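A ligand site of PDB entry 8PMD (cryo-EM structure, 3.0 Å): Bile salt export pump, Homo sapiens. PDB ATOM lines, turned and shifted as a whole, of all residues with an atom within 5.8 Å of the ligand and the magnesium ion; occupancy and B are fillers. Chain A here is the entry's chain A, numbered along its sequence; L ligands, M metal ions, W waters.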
ATOM      1  N   ASP A 191      31.853  21.163  -8.484  1.00  0.00           N
ATOM      2  CA  ASP A 191      32.081  22.108  -7.353  1.00  0.00           C
ATOM      3  C   ASP A 191      33.574  22.427  -7.274  1.00  0.00           C
ATOM      4  O   ASP A 191      33.910  23.583  -6.958  1.00  0.00           O
ATOM      5  CB  ASP A 191      31.544  21.548  -6.028  1.00  0.00           C
ATOM      6  CG  ASP A 191      30.030  21.623  -5.907  1.00  0.00           C
ATOM      7  OD1 ASP A 191      29.358  21.590  -6.962  1.00  0.00           O
ATOM      8  OD2 ASP A 191      29.540  21.719  -4.773  1.00  0.00           O
ATOM      9  N   TYR A 429      30.509  18.662   2.796  1.00  0.00           N
ATOM     10  CA  TYR A 429      30.727  18.982   1.399  1.00  0.00           C
ATOM     11  C   TYR A 429      32.168  18.703   0.988  1.00  0.00           C
ATOM     12  O   TYR A 429      33.087  18.843   1.794  1.00  0.00           O
ATOM     13  CB  TYR A 429      30.389  20.439   1.112  1.00  0.00           C
ATOM     14  CG  TYR A 429      28.950  20.685   0.752  1.00  0.00           C
ATOM     15  CD1 TYR A 429      28.505  20.569  -0.550  1.00  0.00           C
ATOM     16  CD2 TYR A 429      28.031  21.053   1.720  1.00  0.00           C
ATOM     17  CE1 TYR A 429      27.198  20.786  -0.883  1.00  0.00           C
ATOM     18  CE2 TYR A 429      26.719  21.280   1.396  1.00  0.00           C
ATOM     19  CZ  TYR A 429      26.296  21.143   0.095  1.00  0.00           C
ATOM     20  OH  TYR A 429      24.984  21.371  -0.229  1.00  0.00           O
ATOM     21  N   SER A 431      33.887  20.531  -0.888  1.00  0.00           N
ATOM     22  CA  SER A 431      34.581  21.814  -0.912  1.00  0.00           C
ATOM     23  C   SER A 431      35.044  22.244   0.478  1.00  0.00           C
ATOM     24  O   SER A 431      36.089  22.891   0.597  1.00  0.00           O
ATOM     25  CB  SER A 431      33.679  22.878  -1.523  1.00  0.00           C
ATOM     26  OG  SER A 431      34.320  24.145  -1.515  1.00  0.00           O
ATOM     27  N   ARG A 432      34.283  21.906   1.519  1.00  0.00           N
ATOM     28  CA  ARG A 432      34.612  22.265   2.896  1.00  0.00           C
ATOM     29  C   ARG A 432      34.534  21.003   3.735  1.00  0.00           C
ATOM     30  O   ARG A 432      33.561  20.786   4.473  1.00  0.00           O
ATOM     31  CB  ARG A 432      33.679  23.349   3.430  1.00  0.00           C
ATOM     32  CG  ARG A 432      34.368  24.655   3.753  1.00  0.00           C
ATOM     33  CD  ARG A 432      33.393  25.823   3.787  1.00  0.00           C
ATOM     34  NE  ARG A 432      33.237  26.444   2.476  1.00  0.00           N
ATOM     35  CZ  ARG A 432      32.100  26.918   1.992  1.00  0.00           C
ATOM     36  NH1 ARG A 432      30.985  26.874   2.697  1.00  0.00           N
ATOM     37  NH2 ARG A 432      32.084  27.448   0.769  1.00  0.00           N
ATOM     38  N   ILE A 437      28.020  19.301   8.377  1.00  0.00           N
ATOM     39  CA  ILE A 437      26.800  20.027   8.075  1.00  0.00           C
ATOM     40  C   ILE A 437      25.562  19.222   8.433  1.00  0.00           C
ATOM     41  O   ILE A 437      24.604  19.764   8.984  1.00  0.00           O
ATOM     42  CB  ILE A 437      26.813  20.450   6.596  1.00  0.00           C
ATOM     43  CG1 ILE A 437      27.829  21.571   6.395  1.00  0.00           C
ATOM     44  CG2 ILE A 437      25.440  20.886   6.138  1.00  0.00           C
ATOM     45  CD1 ILE A 437      28.135  21.881   4.970  1.00  0.00           C
ATOM     46  N   GLY A 455      13.556  26.140   9.780  1.00  0.00           N
ATOM     47  CA  GLY A 455      14.807  26.339  10.480  1.00  0.00           C
ATOM     48  C   GLY A 455      15.509  27.606  10.035  1.00  0.00           C
ATOM     49  O   GLY A 455      15.097  28.256   9.069  1.00  0.00           O
ATOM     50  N   PRO A 456      16.563  27.975  10.731  1.00  0.00           N
ATOM     51  CA  PRO A 456      17.303  29.189  10.375  1.00  0.00           C
ATOM     52  C   PRO A 456      18.118  28.985   9.097  1.00  0.00           C
ATOM     53  O   PRO A 456      18.216  27.889   8.556  1.00  0.00           O
ATOM     54  CB  PRO A 456      18.209  29.426  11.578  1.00  0.00           C
ATOM     55  CG  PRO A 456      18.400  28.080  12.162  1.00  0.00           C
ATOM     56  CD  PRO A 456      17.122  27.327  11.933  1.00  0.00           C
ATOM     57  N   SER A 457      18.686  30.087   8.619  1.00  0.00           N
ATOM     58  CA  SER A 457      19.565  30.016   7.458  1.00  0.00           C
ATOM     59  C   SER A 457      20.813  29.229   7.796  1.00  0.00           C
ATOM     60  O   SER A 457      21.398  29.375   8.881  1.00  0.00           O
ATOM     61  CB  SER A 457      19.933  31.428   7.001  1.00  0.00           C
ATOM     62  OG  SER A 457      20.940  31.375   6.005  1.00  0.00           O
ATOM     63  N   GLY A 458      21.242  28.384   6.867  1.00  0.00           N
ATOM     64  CA  GLY A 458      22.397  27.530   7.068  1.00  0.00           C
ATOM     65  C   GLY A 458      22.123  26.253   7.823  1.00  0.00           C
ATOM     66  O   GLY A 458      23.067  25.498   8.087  1.00  0.00           O
ATOM     67  N   ALA A 459      20.869  25.976   8.177  1.00  0.00           N
ATOM     68  CA  ALA A 459      20.509  24.793   8.948  1.00  0.00           C
ATOM     69  C   ALA A 459      20.520  23.517   8.127  1.00  0.00           C
ATOM     70  O   ALA A 459      20.040  22.486   8.603  1.00  0.00           O
ATOM     71  CB  ALA A 459      19.136  24.975   9.599  1.00  0.00           C
ATOM     72  N   GLY A 460      21.044  23.561   6.909  1.00  0.00           N
ATOM     73  CA  GLY A 460      21.127  22.367   6.075  1.00  0.00           C
ATOM     74  C   GLY A 460      19.801  21.830   5.579  1.00  0.00           C
ATOM     75  O   GLY A 460      19.565  20.624   5.662  1.00  0.00           O
ATOM     76  N   LYS A 461      18.931  22.693   5.055  1.00  0.00           N
ATOM     77  CA  LYS A 461      17.706  22.222   4.427  1.00  0.00           C
ATOM     78  C   LYS A 461      17.935  21.901   2.951  1.00  0.00           C
ATOM     79  O   LYS A 461      17.542  20.827   2.471  1.00  0.00           O
ATOM     80  CB  LYS A 461      16.613  23.272   4.594  1.00  0.00           C
ATOM     81  CG  LYS A 461      16.447  23.762   6.027  1.00  0.00           C
ATOM     82  CD  LYS A 461      15.367  24.824   6.156  1.00  0.00           C
ATOM     83  CE  LYS A 461      15.848  26.169   5.647  1.00  0.00           C
ATOM     84  NZ  LYS A 461      17.008  26.666   6.433  1.00  0.00           N
ATOM     85  N   SER A 462      18.572  22.811   2.217  1.00  0.00           N
ATOM     86  CA  SER A 462      18.925  22.540   0.836  1.00  0.00           C
ATOM     87  C   SER A 462      19.910  21.389   0.702  1.00  0.00           C
ATOM     88  O   SER A 462      19.920  20.711  -0.321  1.00  0.00           O
ATOM     89  CB  SER A 462      19.512  23.802   0.188  1.00  0.00           C
ATOM     90  OG  SER A 462      18.586  24.870   0.222  1.00  0.00           O
ATOM     91  N   THR A 463      20.736  21.144   1.730  1.00  0.00           N
ATOM     92  CA  THR A 463      21.636  19.993   1.669  1.00  0.00           C
ATOM     93  C   THR A 463      20.853  18.689   1.688  1.00  0.00           C
ATOM     94  O   THR A 463      21.143  17.774   0.909  1.00  0.00           O
ATOM     95  CB  THR A 463      22.621  20.024   2.827  1.00  0.00           C
ATOM     96  OG1 THR A 463      21.908  20.140   4.057  1.00  0.00           O
ATOM     97  CG2 THR A 463      23.574  21.189   2.689  1.00  0.00           C
ATOM     98  N   ALA A 464      19.863  18.578   2.569  1.00  0.00           N
ATOM     99  CA  ALA A 464      19.004  17.385   2.558  1.00  0.00           C
ATOM    100  C   ALA A 464      18.247  17.289   1.246  1.00  0.00           C
ATOM    101  O   ALA A 464      18.074  16.199   0.687  1.00  0.00           O
ATOM    102  CB  ALA A 464      18.037  17.425   3.735  1.00  0.00           C
ATOM    103  N   GLN A 466      19.232  18.268  -1.696  1.00  0.00           N
ATOM    104  CA  GLN A 466      20.148  17.752  -2.719  1.00  0.00           C
ATOM    105  C   GLN A 466      20.515  16.296  -2.460  1.00  0.00           C
ATOM    106  O   GLN A 466      20.737  15.541  -3.414  1.00  0.00           O
ATOM    107  CB  GLN A 466      21.408  18.609  -2.766  1.00  0.00           C
ATOM    108  CG  GLN A 466      21.176  20.041  -3.220  1.00  0.00           C
ATOM    109  CD  GLN A 466      22.436  20.871  -3.205  1.00  0.00           C
ATOM    110  OE1 GLN A 466      23.440  20.518  -3.830  1.00  0.00           O
ATOM    111  NE2 GLN A 466      22.408  21.987  -2.479  1.00  0.00           N
ATOM    112  N   TYR A 472      24.769  14.111  -3.963  1.00  0.00           N
ATOM    113  CA  TYR A 472      25.904  13.643  -3.198  1.00  0.00           C
ATOM    114  C   TYR A 472      25.518  12.342  -2.504  1.00  0.00           C
ATOM    115  O   TYR A 472      24.374  11.899  -2.554  1.00  0.00           O
ATOM    116  CB  TYR A 472      26.358  14.680  -2.159  1.00  0.00           C
ATOM    117  CG  TYR A 472      26.752  16.017  -2.731  1.00  0.00           C
ATOM    118  CD1 TYR A 472      25.800  16.961  -3.078  1.00  0.00           C
ATOM    119  CD2 TYR A 472      28.089  16.344  -2.902  1.00  0.00           C
ATOM    120  CE1 TYR A 472      26.164  18.189  -3.585  1.00  0.00           C
ATOM    121  CE2 TYR A 472      28.462  17.571  -3.415  1.00  0.00           C
ATOM    122  OH  TYR A 472      27.875  19.715  -4.261  1.00  0.00           O
ATOM    123  N   GLN A 503      16.187  27.084  -5.200  1.00  0.00           N
ATOM    124  CA  GLN A 503      15.993  28.335  -4.479  1.00  0.00           C
ATOM    125  C   GLN A 503      15.879  29.488  -5.455  1.00  0.00           C
ATOM    126  O   GLN A 503      15.101  30.419  -5.236  1.00  0.00           O
ATOM    127  CB  GLN A 503      17.128  28.560  -3.475  1.00  0.00           C
ATOM    128  CG  GLN A 503      16.774  29.532  -2.374  1.00  0.00           C
ATOM    129  CD  GLN A 503      17.166  29.057  -0.994  1.00  0.00           C
ATOM    130  OE1 GLN A 503      17.662  27.946  -0.819  1.00  0.00           O
ATOM    131  NE2 GLN A 503      16.959  29.914   0.004  1.00  0.00           N
ATOM    132  N   ASP A 583      11.620  24.329  -2.814  1.00  0.00           N
ATOM    133  CA  ASP A 583      12.603  25.110  -2.075  1.00  0.00           C
ATOM    134  C   ASP A 583      12.218  26.582  -2.195  1.00  0.00           C
ATOM    135  O   ASP A 583      12.625  27.274  -3.127  1.00  0.00           O
ATOM    136  CB  ASP A 583      14.022  24.856  -2.602  1.00  0.00           C
ATOM    137  OD1 ASP A 583      14.836  26.040  -0.707  1.00  0.00           O
ATOM    138  OD2 ASP A 583      16.213  24.655  -1.707  1.00  0.00           O
ATOM    139  N   VAL A 613      10.247  23.477   1.973  1.00  0.00           N
ATOM    140  CA  VAL A 613      10.876  24.252   3.035  1.00  0.00           C
ATOM    141  C   VAL A 613      10.165  25.590   3.139  1.00  0.00           C
ATOM    142  O   VAL A 613       9.886  26.234   2.121  1.00  0.00           O
ATOM    143  CB  VAL A 613      12.387  24.430   2.790  1.00  0.00           C
ATOM    144  CG1 VAL A 613      13.098  23.088   2.802  1.00  0.00           C
ATOM    145  CG2 VAL A 613      12.642  25.136   1.479  1.00  0.00           C
ATOM    146  N   HIS A 615       9.513  29.350   5.608  1.00  0.00           N
ATOM    147  CA  HIS A 615       9.902  30.269   6.659  1.00  0.00           C
ATOM    148  C   HIS A 615       8.722  31.006   7.275  1.00  0.00           C
ATOM    149  O   HIS A 615       8.893  31.669   8.306  1.00  0.00           O
ATOM    150  CB  HIS A 615      10.903  31.310   6.125  1.00  0.00           C
ATOM    151  CG  HIS A 615      12.321  30.855   6.165  1.00  0.00           C
ATOM    152  ND1 HIS A 615      13.384  31.720   6.350  1.00  0.00           N
ATOM    153  CD2 HIS A 615      12.873  29.625   6.034  1.00  0.00           C
ATOM    154  CE1 HIS A 615      14.509  31.040   6.339  1.00  0.00           C
ATOM    155  NE2 HIS A 615      14.231  29.770   6.155  1.00  0.00           N
ATOM    156  N   ARG A 948      23.442  21.884 -12.163  1.00  0.00           N
ATOM    157  CA  ARG A 948      22.454  21.468 -11.167  1.00  0.00           C
ATOM    158  C   ARG A 948      21.048  21.480 -11.737  1.00  0.00           C
ATOM    159  O   ARG A 948      20.261  20.549 -11.486  1.00  0.00           O
ATOM    160  CB  ARG A 948      22.559  22.372  -9.943  1.00  0.00           C
ATOM    161  CG  ARG A 948      23.848  22.189  -9.170  1.00  0.00           C
ATOM    162  CD  ARG A 948      24.338  23.491  -8.557  1.00  0.00           C
ATOM    163  NE  ARG A 948      25.370  23.291  -7.548  1.00  0.00           N
ATOM    164  CZ  ARG A 948      25.204  22.624  -6.405  1.00  0.00           C
ATOM    165  NH1 ARG A 948      24.034  22.113  -6.065  1.00  0.00           N
ATOM    166  NH2 ARG A 948      26.242  22.481  -5.586  1.00  0.00           N
ATOM    167  N   PHE A1200      28.284  33.321  12.003  1.00  0.00           N
ATOM    168  CA  PHE A1200      28.410  32.221  11.050  1.00  0.00           C
ATOM    169  C   PHE A1200      29.820  32.160  10.456  1.00  0.00           C
ATOM    170  O   PHE A1200      30.401  31.085  10.345  1.00  0.00           O
ATOM    171  CB  PHE A1200      27.369  32.363   9.943  1.00  0.00           C
ATOM    172  CG  PHE A1200      27.779  31.735   8.640  1.00  0.00           C
ATOM    173  CD1 PHE A1200      27.757  30.365   8.486  1.00  0.00           C
ATOM    174  CD2 PHE A1200      28.199  32.523   7.580  1.00  0.00           C
ATOM    175  CE1 PHE A1200      28.139  29.785   7.283  1.00  0.00           C
ATOM    176  CE2 PHE A1200      28.576  31.953   6.386  1.00  0.00           C
ATOM    177  CZ  PHE A1200      28.554  30.583   6.232  1.00  0.00           C
ATOM    178  N   LEU A1204      33.380  29.291  10.809  1.00  0.00           N
ATOM    179  CA  LEU A1204      34.061  28.589   9.729  1.00  0.00           C
ATOM    180  C   LEU A1204      35.502  28.267  10.104  1.00  0.00           C
ATOM    181  O   LEU A1204      36.120  28.993  10.892  1.00  0.00           O
ATOM    182  CB  LEU A1204      34.039  29.430   8.461  1.00  0.00           C
ATOM    183  CG  LEU A1204      32.696  29.538   7.748  1.00  0.00           C
ATOM    184  CD1 LEU A1204      32.806  30.446   6.530  1.00  0.00           C
ATOM    185  CD2 LEU A1204      32.171  28.164   7.357  1.00  0.00           C
ATOM    186  N   SER A1217      28.068  30.071  -5.099  1.00  0.00           N
ATOM    187  CA  SER A1217      27.113  28.969  -5.051  1.00  0.00           C
ATOM    188  C   SER A1217      27.426  27.948  -3.968  1.00  0.00           C
ATOM    189  O   SER A1217      26.600  27.062  -3.732  1.00  0.00           O
ATOM    190  CB  SER A1217      27.055  28.266  -6.407  1.00  0.00           C
ATOM    191  OG  SER A1217      28.339  28.264  -7.024  1.00  0.00           O
ATOM    192  N   GLN A1218      28.575  28.045  -3.318  1.00  0.00           N
ATOM    193  CA  GLN A1218      28.938  27.126  -2.249  1.00  0.00           C
ATOM    194  C   GLN A1218      28.500  27.618  -0.874  1.00  0.00           C
ATOM    195  O   GLN A1218      29.117  27.260   0.143  1.00  0.00           O
ATOM    196  CB  GLN A1218      30.443  26.850  -2.273  1.00  0.00           C
ATOM    197  CG  GLN A1218      30.868  25.933  -3.404  1.00  0.00           C
ATOM    198  CD  GLN A1218      32.369  25.913  -3.613  1.00  0.00           C
ATOM    199  NE2 GLN A1218      32.798  25.436  -4.776  1.00  0.00           N
ATOM    200  N   LEU A1219      27.465  28.441  -0.820  1.00  0.00           N
ATOM    201  CA  LEU A1219      26.842  28.876   0.422  1.00  0.00           C
ATOM    202  C   LEU A1219      25.339  28.729   0.275  1.00  0.00           C
ATOM    203  O   LEU A1219      24.801  28.677  -0.827  1.00  0.00           O
ATOM    204  CB  LEU A1219      27.187  30.333   0.756  1.00  0.00           C
ATOM    205  CG  LEU A1219      28.654  30.749   0.795  1.00  0.00           C
ATOM    206  CD1 LEU A1219      28.831  32.096   0.100  1.00  0.00           C
ATOM    207  CD2 LEU A1219      29.154  30.819   2.233  1.00  0.00           C
ATOM    208  N   SER A1220      24.657  28.652   1.416  1.00  0.00           N
ATOM    209  CA  SER A1220      23.204  28.756   1.365  1.00  0.00           C
ATOM    210  C   SER A1220      22.816  30.179   0.965  1.00  0.00           C
ATOM    211  O   SER A1220      23.583  31.126   1.117  1.00  0.00           O
ATOM    212  CB  SER A1220      22.582  28.382   2.712  1.00  0.00           C
ATOM    213  OG  SER A1220      22.267  29.538   3.465  1.00  0.00           O
ATOM    214  N   ARG A1221      21.606  30.300   0.424  1.00  0.00           N
ATOM    215  CA  ARG A1221      21.199  31.571  -0.169  1.00  0.00           C
ATOM    216  C   ARG A1221      21.037  32.666   0.879  1.00  0.00           C
ATOM    217  O   ARG A1221      21.184  33.859   0.561  1.00  0.00           O
ATOM    218  CB  ARG A1221      19.917  31.389  -0.959  1.00  0.00           C
ATOM    219  CG  ARG A1221      20.170  31.187  -2.437  1.00  0.00           C
ATOM    220  CD  ARG A1221      20.752  29.805  -2.722  1.00  0.00           C
ATOM    221  NE  ARG A1221      21.421  29.743  -4.011  1.00  0.00           N
ATOM    222  NH1 ARG A1221      23.567  29.944  -3.147  1.00  0.00           N
ATOM    223  NH2 ARG A1221      23.245  29.739  -5.413  1.00  0.00           N
ATOM    224  N   GLY A1222      20.730  32.297   2.123  1.00  0.00           N
ATOM    225  CA  GLY A1222      20.658  33.297   3.179  1.00  0.00           C
ATOM    226  C   GLY A1222      21.972  34.010   3.415  1.00  0.00           C
ATOM    227  O   GLY A1222      22.006  35.230   3.558  1.00  0.00           O
ATOM    228  N   GLU A1223      23.073  33.256   3.436  1.00  0.00           N
ATOM    229  CA  GLU A1223      24.365  33.903   3.629  1.00  0.00           C
ATOM    230  C   GLU A1223      24.796  34.681   2.398  1.00  0.00           C
ATOM    231  O   GLU A1223      25.520  35.673   2.511  1.00  0.00           O
ATOM    232  CB  GLU A1223      25.440  32.883   4.016  1.00  0.00           C
ATOM    233  CG  GLU A1223      25.102  32.054   5.254  1.00  0.00           C
ATOM    234  OE1 GLU A1223      24.500  30.407   3.704  1.00  0.00           O
ATOM    235  OE2 GLU A1223      24.647  29.793   5.798  1.00  0.00           O
ATOM    236  N   ALA A1248      15.509  35.395   1.114  1.00  0.00           N
ATOM    237  CA  ALA A1248      16.023  34.144   1.648  1.00  0.00           C
ATOM    238  C   ALA A1248      16.012  34.117   3.173  1.00  0.00           C
ATOM    239  O   ALA A1248      15.470  33.193   3.778  1.00  0.00           O
ATOM    240  CB  ALA A1248      17.442  33.890   1.121  1.00  0.00           C
HETATM  241  P1  LIG L   1      18.849  28.924   3.442  1.00  0.00           P
HETATM  242  O1  LIG L   1      19.680  30.156   3.362  1.00  0.00           O
HETATM  243  O2  LIG L   1      17.631  29.050   4.352  1.00  0.00           O
HETATM  244  O3  LIG L   1      18.392  28.399   2.079  1.00  0.00           O
HETATM  245  P2  LIG L   1      19.611  26.153   4.245  1.00  0.00           P
HETATM  246  O4  LIG L   1      19.084  25.786   5.571  1.00  0.00           O
HETATM  247  O5  LIG L   1      18.818  25.607   3.067  1.00  0.00           O
HETATM  248  O6  LIG L   1      19.692  27.718   4.059  1.00  0.00           O
HETATM  249  P3  LIG L   1      21.946  24.857   2.997  1.00  0.00           P
HETATM  250  O7  LIG L   1      21.490  23.445   3.029  1.00  0.00           O
HETATM  251  O8  LIG L   1      21.816  25.534   1.643  1.00  0.00           O
HETATM  252  O9  LIG L   1      21.126  25.722   4.036  1.00  0.00           O
HETATM  253  O10 LIG L   1      23.433  25.002   3.480  1.00  0.00           O
HETATM  254  C1  LIG L   1      23.812  24.766   4.851  1.00  0.00           C
HETATM  255  C2  LIG L   1      25.296  24.902   4.988  1.00  0.00           C
HETATM  256  O11 LIG L   1      25.956  24.230   3.886  1.00  0.00           O
HETATM  257  C3  LIG L   1      25.831  26.333   5.004  1.00  0.00           C
HETATM  258  O12 LIG L   1      26.827  26.497   6.005  1.00  0.00           O
HETATM  259  C4  LIG L   1      26.417  26.505   3.597  1.00  0.00           C
HETATM  260  O13 LIG L   1      27.499  27.422   3.595  1.00  0.00           O
HETATM  261  C5  LIG L   1      26.914  25.096   3.315  1.00  0.00           C
HETATM  262  N1  LIG L   1      27.048  24.763   1.897  1.00  0.00           N
HETATM  263  C6  LIG L   1      26.048  24.658   0.975  1.00  0.00           C
HETATM  264  N2  LIG L   1      26.455  24.337  -0.233  1.00  0.00           N
HETATM  265  C7  LIG L   1      27.826  24.233  -0.084  1.00  0.00           C
HETATM  266  C8  LIG L   1      28.857  23.926  -0.996  1.00  0.00           C
HETATM  267  N3  LIG L   1      28.653  23.652  -2.282  1.00  0.00           N
HETATM  268  N4  LIG L   1      30.125  23.897  -0.532  1.00  0.00           N
HETATM  269  C9  LIG L   1      30.345  24.173   0.760  1.00  0.00           C
HETATM  270  N5  LIG L   1      29.456  24.479   1.711  1.00  0.00           N
HETATM  271  C10 LIG L   1      28.207  24.487   1.223  1.00  0.00           C
HETATM  272 MG    MG M   1      17.965  26.824   0.873  1.00  0.00          MG
HETATM  273  O   HOH W   1      19.949  27.079   0.405  1.00  0.00           O
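An oxygen (O5) of the ligand sits at hydrogen-bond distance from the backbone NH of Ser 462 (2.9 Å). N of Lys 461 is in hydrogen-bond range of O4 of the ligand (3.1 Å). An oxygen (O4) of the ligand lies within salt-bridge range of the side-chain amino group of Lys 461, at 2.4 Å. An oxygen (O1) of the ligand sits at hydrogen-bond distance from the side-chain hydroxyl (OG) of Ser 1220, at 2.7 Å. O1 of the ligand lies within hydrogen-bond range of N of Gly 1222 (2.7 Å). The backbone NH (N) of Thr 463 is in hydrogen-bond range of an oxygen (O7) of the ligand. The side-chain hydroxyl (OG1) of Thr 463 lies close to an oxygen (O7) of the ligand (3.5 Å). NH1 of Arg 432 is in hydrogen-bond range of N5 of the ligand (3.0 Å). The backbone NH (N) of Ala 459 sits at hydrogen-bond distance from an oxygen (O4) of the ligand. The side-chain hydroxyl (OG) of Ser 457 sits at hydrogen-bond distance from an oxygen (O1) of the ligand (3.2 Å). OH of Tyr 429 sits close to N2 of the ligand (3.3 Å). An oxygen (O4) of the ligand is in hydrogen-bond range of the backbone NH of Gly 460 (3.3 Å). OD2 of Asp 191 sits at hydrogen-bond distance from N3 of the ligand, at 3.3 Å. The backbone NH (N) of Gly 458 is in hydrogen-bond range of an oxygen (O6) of the ligand (3.3 Å).
The side-chain carboxylate (OD1) of Asp 583 lies close to the side-chain amide oxygen (OE1) of Gln 503 (3.4 Å). The side-chain carboxylate (OD2) of Asp 583 sits close to the side-chain hydroxyl (OG) of Ser 462, at 3.1 Å. The side-chain hydroxyl of Ser 457 is in hydrogen-bond range of the side-chain hydroxyl of Ser 1220, 3.4 Å away. The side-chain carboxylate (OE1) of Glu 1223 is in hydrogen-bond range of the side-chain hydroxyl (OG) of Ser 1220 (2.4 Å). O of Gly 460 sits at hydrogen-bond distance from OG1 of Thr 463 (2.9 Å). NH2 of Arg 432 lies within hydrogen-bond range of O of Gln 1218 (3.0 Å). The side-chain carboxylate (OD2) of Asp 191 is in salt-bridge range of the guanidinium group (NH2) of Arg 948, 3.5 Å away. O of Gly 455 is in hydrogen-bond range of NE2 of His 615.
The backbone carbonyl oxygen (O) of Gln 1218 sits close to a nitrogen (N5) of the ligand, 3.2 Å away. Ser 431 touches the ligand (CB to N4, 3.8 Å). Ile 437 touches the ligand (CD1 to O11, 3.4 Å). Pro 456 touches the ligand. His 615 touches the ligand (NE2 to O2, 3.9 Å). Phe 1200 touches the ligand (CE1 to O12, 3.8 Å). CA of Leu 1219 touches O13 of the ligand, at 3.6 Å. N of Arg 1221 touches O1 of the ligand, at 3.5 Å. Glu 1223 touches the ligand (OE2 to C3, 3.7 Å). Hydrophobic or aromatic side chains within 4 Å of the ligand: Tyr 429, Ile 437 and Phe 1200. 22 residues have an atom within 4 Å of the ligand: Asp 191, Tyr 429, Ser 431, Arg 432, Ile 437, Pro 456, Ser 457, Gly 458, Ala 459, Gly 460, Lys 461, Ser 462, Thr 463, Gln 503, His 615, Phe 1200, Gln 1218, Leu 1219, Ser 1220, Arg 1221, Gly 1222 and Glu 1223. The nearest printed residue that does not touch the ligand is Ser 1217 (4.2 Å).
OD1 of Asp 583 touches the magnesium ion (3.6 Å). Of the 32 residues printed, 3 come within 4 Å of the magnesium ion. The nearest printed residue that does not touch the magnesium ion is Arg 1221 (5.1 Å).
The magnesium ion is bound by an oxygen (O3) of the ligand, the side-chain amide oxygen of Gln 503, water W1 and the side-chain hydroxyl of Ser 462. Slightly farther from the magnesium ion lies an oxygen (O5) of the ligand (2.6 Å).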
